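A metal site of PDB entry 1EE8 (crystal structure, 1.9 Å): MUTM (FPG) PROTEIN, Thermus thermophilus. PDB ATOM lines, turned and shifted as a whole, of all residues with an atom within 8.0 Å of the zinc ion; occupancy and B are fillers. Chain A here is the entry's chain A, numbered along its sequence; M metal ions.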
ATOM      1  N   PHE A 169      -1.469 -15.109 -13.009  1.00  0.00           N
ATOM      2  CA  PHE A 169      -0.341 -15.636 -12.255  1.00  0.00           C
ATOM      3  C   PHE A 169      -0.828 -16.260 -10.967  1.00  0.00           C
ATOM      4  O   PHE A 169      -0.395 -17.348 -10.583  1.00  0.00           O
ATOM      5  CB  PHE A 169       0.661 -14.547 -11.870  1.00  0.00           C
ATOM      6  CG  PHE A 169       1.734 -15.045 -10.947  1.00  0.00           C
ATOM      7  CD1 PHE A 169       2.797 -15.800 -11.442  1.00  0.00           C
ATOM      8  CD2 PHE A 169       1.643 -14.843  -9.577  1.00  0.00           C
ATOM      9  CE1 PHE A 169       3.739 -16.340 -10.583  1.00  0.00           C
ATOM     10  CE2 PHE A 169       2.581 -15.381  -8.709  1.00  0.00           C
ATOM     11  CZ  PHE A 169       3.634 -16.128  -9.210  1.00  0.00           C
ATOM     12  N   ARG A 172      -2.084 -19.437 -11.654  1.00  0.00           N
ATOM     13  CA  ARG A 172      -1.086 -20.284 -12.309  1.00  0.00           C
ATOM     14  C   ARG A 172      -1.584 -20.824 -13.649  1.00  0.00           C
ATOM     15  O   ARG A 172      -1.502 -22.022 -13.919  1.00  0.00           O
ATOM     16  CB  ARG A 172      -0.698 -21.441 -11.388  1.00  0.00           C
ATOM     17  CG  ARG A 172      -0.115 -21.005 -10.045  1.00  0.00           C
ATOM     18  CD  ARG A 172       1.211 -20.271 -10.221  1.00  0.00           C
ATOM     19  NE  ARG A 172       1.939 -20.143  -8.960  1.00  0.00           N
ATOM     20  CZ  ARG A 172       1.669 -19.259  -8.001  1.00  0.00           C
ATOM     21  NH1 ARG A 172       0.684 -18.374  -8.141  1.00  0.00           N
ATOM     22  NH2 ARG A 172       2.388 -19.263  -6.879  1.00  0.00           N
ATOM     23  N   VAL A 230       4.007 -10.352 -11.274  1.00  0.00           N
ATOM     24  CA  VAL A 230       4.593 -10.353 -12.602  1.00  0.00           C
ATOM     25  C   VAL A 230       4.448  -9.063 -13.400  1.00  0.00           C
ATOM     26  O   VAL A 230       5.327  -8.746 -14.210  1.00  0.00           O
ATOM     27  CB  VAL A 230       4.018 -11.518 -13.448  1.00  0.00           C
ATOM     28  CG1 VAL A 230       4.309 -12.862 -12.755  1.00  0.00           C
ATOM     29  CG2 VAL A 230       2.522 -11.328 -13.635  1.00  0.00           C
ATOM     30  N   PRO A 237      12.889 -11.745 -10.572  1.00  0.00           N
ATOM     31  CA  PRO A 237      12.572 -13.087 -10.088  1.00  0.00           C
ATOM     32  C   PRO A 237      11.098 -13.341  -9.770  1.00  0.00           C
ATOM     33  O   PRO A 237      10.466 -12.548  -9.079  1.00  0.00           O
ATOM     34  CB  PRO A 237      13.427 -13.223  -8.816  1.00  0.00           C
ATOM     35  CG  PRO A 237      14.513 -12.204  -8.998  1.00  0.00           C
ATOM     36  CD  PRO A 237      13.781 -11.055  -9.613  1.00  0.00           C
ATOM     37  N   CYS A 238      10.556 -14.446 -10.287  1.00  0.00           N
ATOM     38  CA  CYS A 238       9.181 -14.805  -9.973  1.00  0.00           C
ATOM     39  C   CYS A 238       9.162 -14.950  -8.453  1.00  0.00           C
ATOM     40  O   CYS A 238      10.129 -15.414  -7.864  1.00  0.00           O
ATOM     41  CB  CYS A 238       8.815 -16.139 -10.643  1.00  0.00           C
ATOM     42  SG  CYS A 238       7.289 -16.904 -10.033  1.00  0.00           S
ATOM     43  N   PRO A 239       8.063 -14.553  -7.803  1.00  0.00           N
ATOM     44  CA  PRO A 239       8.060 -14.689  -6.333  1.00  0.00           C
ATOM     45  C   PRO A 239       7.796 -16.120  -5.852  1.00  0.00           C
ATOM     46  O   PRO A 239       7.889 -16.404  -4.663  1.00  0.00           O
ATOM     47  CB  PRO A 239       6.970 -13.719  -5.918  1.00  0.00           C
ATOM     48  CG  PRO A 239       5.976 -13.857  -7.030  1.00  0.00           C
ATOM     49  CD  PRO A 239       6.852 -13.853  -8.266  1.00  0.00           C
ATOM     50  N   ALA A 240       7.464 -17.011  -6.784  1.00  0.00           N
ATOM     51  CA  ALA A 240       7.183 -18.389  -6.410  1.00  0.00           C
ATOM     52  C   ALA A 240       8.299 -19.383  -6.732  1.00  0.00           C
ATOM     53  O   ALA A 240       8.557 -20.301  -5.950  1.00  0.00           O
ATOM     54  CB  ALA A 240       5.881 -18.848  -7.078  1.00  0.00           C
ATOM     55  N   CYS A 241       8.965 -19.200  -7.872  1.00  0.00           N
ATOM     56  CA  CYS A 241      10.039 -20.125  -8.270  1.00  0.00           C
ATOM     57  C   CYS A 241      11.390 -19.458  -8.509  1.00  0.00           C
ATOM     58  O   CYS A 241      12.365 -20.143  -8.825  1.00  0.00           O
ATOM     59  CB  CYS A 241       9.634 -20.866  -9.540  1.00  0.00           C
ATOM     60  SG  CYS A 241       9.730 -19.856 -11.015  1.00  0.00           S
ATOM     61  N   GLY A 242      11.444 -18.140  -8.356  1.00  0.00           N
ATOM     62  CA  GLY A 242      12.692 -17.419  -8.549  1.00  0.00           C
ATOM     63  C   GLY A 242      13.185 -17.260  -9.983  1.00  0.00           C
ATOM     64  O   GLY A 242      14.215 -16.625 -10.211  1.00  0.00           O
ATOM     65  N   ARG A 243      12.477 -17.838 -10.948  1.00  0.00           N
ATOM     66  CA  ARG A 243      12.873 -17.724 -12.355  1.00  0.00           C
ATOM     67  C   ARG A 243      12.535 -16.330 -12.880  1.00  0.00           C
ATOM     68  O   ARG A 243      11.635 -15.666 -12.365  1.00  0.00           O
ATOM     69  CB  ARG A 243      12.166 -18.797 -13.187  1.00  0.00           C
ATOM     70  CG  ARG A 243      12.453 -18.687 -14.681  1.00  0.00           C
ATOM     71  CD  ARG A 243      11.770 -19.787 -15.508  1.00  0.00           C
ATOM     72  NE  ARG A 243      12.027 -19.590 -16.934  1.00  0.00           N
ATOM     73  CZ  ARG A 243      11.615 -20.414 -17.891  1.00  0.00           C
ATOM     74  NH1 ARG A 243      11.888 -20.142 -19.163  1.00  0.00           N
ATOM     75  NH2 ARG A 243      10.928 -21.499 -17.580  1.00  0.00           N
ATOM     76  N   PRO A 244      13.273 -15.857 -13.903  1.00  0.00           N
ATOM     77  CA  PRO A 244      13.036 -14.532 -14.493  1.00  0.00           C
ATOM     78  C   PRO A 244      11.659 -14.347 -15.137  1.00  0.00           C
ATOM     79  O   PRO A 244      11.278 -15.091 -16.045  1.00  0.00           O
ATOM     80  CB  PRO A 244      14.152 -14.406 -15.529  1.00  0.00           C
ATOM     81  CG  PRO A 244      15.267 -15.212 -14.915  1.00  0.00           C
ATOM     82  CD  PRO A 244      14.529 -16.437 -14.405  1.00  0.00           C
ATOM     83  N   VAL A 245      10.914 -13.338 -14.682  1.00  0.00           N
ATOM     84  CA  VAL A 245       9.595 -13.060 -15.236  1.00  0.00           C
ATOM     85  C   VAL A 245       9.757 -12.621 -16.689  1.00  0.00           C
ATOM     86  O   VAL A 245      10.616 -11.789 -17.007  1.00  0.00           O
ATOM     87  CB  VAL A 245       8.876 -11.950 -14.453  1.00  0.00           C
ATOM     88  CG1 VAL A 245       7.578 -11.583 -15.151  1.00  0.00           C
ATOM     89  CG2 VAL A 245       8.607 -12.399 -13.029  1.00  0.00           C
ATOM     90  N   PHE A 257       4.316 -12.752 -17.230  1.00  0.00           N
ATOM     91  CA  PHE A 257       4.011 -14.086 -16.721  1.00  0.00           C
ATOM     92  C   PHE A 257       5.278 -14.877 -16.424  1.00  0.00           C
ATOM     93  O   PHE A 257       6.360 -14.533 -16.907  1.00  0.00           O
ATOM     94  CB  PHE A 257       3.209 -14.852 -17.770  1.00  0.00           C
ATOM     95  CG  PHE A 257       4.024 -15.232 -18.976  1.00  0.00           C
ATOM     96  CD1 PHE A 257       4.500 -16.527 -19.144  1.00  0.00           C
ATOM     97  CD2 PHE A 257       4.374 -14.261 -19.924  1.00  0.00           C
ATOM     98  CE1 PHE A 257       5.308 -16.865 -20.231  1.00  0.00           C
ATOM     99  CE2 PHE A 257       5.191 -14.588 -21.010  1.00  0.00           C
ATOM    100  CZ  PHE A 257       5.651 -15.890 -21.161  1.00  0.00           C
ATOM    101  N   CYS A 258       5.135 -15.935 -15.616  1.00  0.00           N
ATOM    102  CA  CYS A 258       6.262 -16.809 -15.301  1.00  0.00           C
ATOM    103  C   CYS A 258       6.015 -18.035 -16.157  1.00  0.00           C
ATOM    104  O   CYS A 258       5.007 -18.735 -15.983  1.00  0.00           O
ATOM    105  CB  CYS A 258       6.271 -17.215 -13.832  1.00  0.00           C
ATOM    106  SG  CYS A 258       7.518 -18.509 -13.463  1.00  0.00           S
ATOM    107  N   PRO A 259       6.934 -18.313 -17.104  1.00  0.00           N
ATOM    108  CA  PRO A 259       6.776 -19.480 -17.970  1.00  0.00           C
ATOM    109  C   PRO A 259       6.613 -20.775 -17.183  1.00  0.00           C
ATOM    110  O   PRO A 259       5.688 -21.561 -17.440  1.00  0.00           O
ATOM    111  CB  PRO A 259       8.059 -19.459 -18.806  1.00  0.00           C
ATOM    112  CG  PRO A 259       8.386 -17.984 -18.876  1.00  0.00           C
ATOM    113  CD  PRO A 259       8.143 -17.555 -17.453  1.00  0.00           C
ATOM    114  N   THR A 260       7.498 -21.002 -16.219  1.00  0.00           N
ATOM    115  CA  THR A 260       7.419 -22.227 -15.436  1.00  0.00           C
ATOM    116  C   THR A 260       6.137 -22.335 -14.614  1.00  0.00           C
ATOM    117  O   THR A 260       5.388 -23.288 -14.753  1.00  0.00           O
ATOM    118  CB  THR A 260       8.617 -22.380 -14.486  1.00  0.00           C
ATOM    119  OG1 THR A 260       9.825 -22.389 -15.245  1.00  0.00           O
ATOM    120  CG2 THR A 260       8.504 -23.694 -13.707  1.00  0.00           C
ATOM    121  N   CYS A 261       5.893 -21.350 -13.756  1.00  0.00           N
ATOM    122  CA  CYS A 261       4.703 -21.377 -12.904  1.00  0.00           C
ATOM    123  C   CYS A 261       3.361 -21.291 -13.622  1.00  0.00           C
ATOM    124  O   CYS A 261       2.345 -21.694 -13.078  1.00  0.00           O
ATOM    125  CB  CYS A 261       4.778 -20.248 -11.874  1.00  0.00           C
ATOM    126  SG  CYS A 261       6.045 -20.503 -10.631  1.00  0.00           S
ATOM    127  N   GLN A 262       3.363 -20.777 -14.847  1.00  0.00           N
ATOM    128  CA  GLN A 262       2.106 -20.646 -15.586  1.00  0.00           C
ATOM    129  C   GLN A 262       1.952 -21.533 -16.811  1.00  0.00           C
ATOM    130  O   GLN A 262       1.281 -21.172 -17.786  1.00  0.00           O
ATOM    131  CB  GLN A 262       1.885 -19.172 -15.939  1.00  0.00           C
ATOM    132  CG  GLN A 262       1.609 -18.318 -14.702  1.00  0.00           C
ATOM    133  CD  GLN A 262       1.494 -16.836 -14.993  1.00  0.00           C
ATOM    134  OE1 GLN A 262       2.492 -16.104 -15.003  1.00  0.00           O
ATOM    135  NE2 GLN A 262       0.268 -16.373 -15.244  1.00  0.00           N
HETATM  136 ZN    ZN M   1       7.607 -18.934 -11.166  1.00  0.00          ZN
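SG of Cys 241 sits close to N of Arg 243 (3.4 Å). SG of Cys 258 lies close to N of Thr 260. The backbone NH (N) of Cys 258 sits at hydrogen-bond distance from the side-chain amide oxygen (OE1) of Gln 262 (2.7 Å). N of Ala 240 sits close to SG of Cys 238. The backbone carbonyl oxygen of Arg 243 lies within hydrogen-bond range of the backbone NH of Cys 238 (2.6 Å).
Of the 18 residues printed, 4 come within 4 Å of the zinc ion. The nearest printed residue that does not touch the zinc ion is Ala 240 (4.4 Å).
SG of Cys 261 binds the zinc ion. The zinc ion is bound by SG of Cys 241 (2.3 Å). The zinc ion is bound by SG of Cys 258 (2.3 Å). The side-chain sulfur (SG) of Cys 238 is bound to the zinc ion (2.3 Å).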
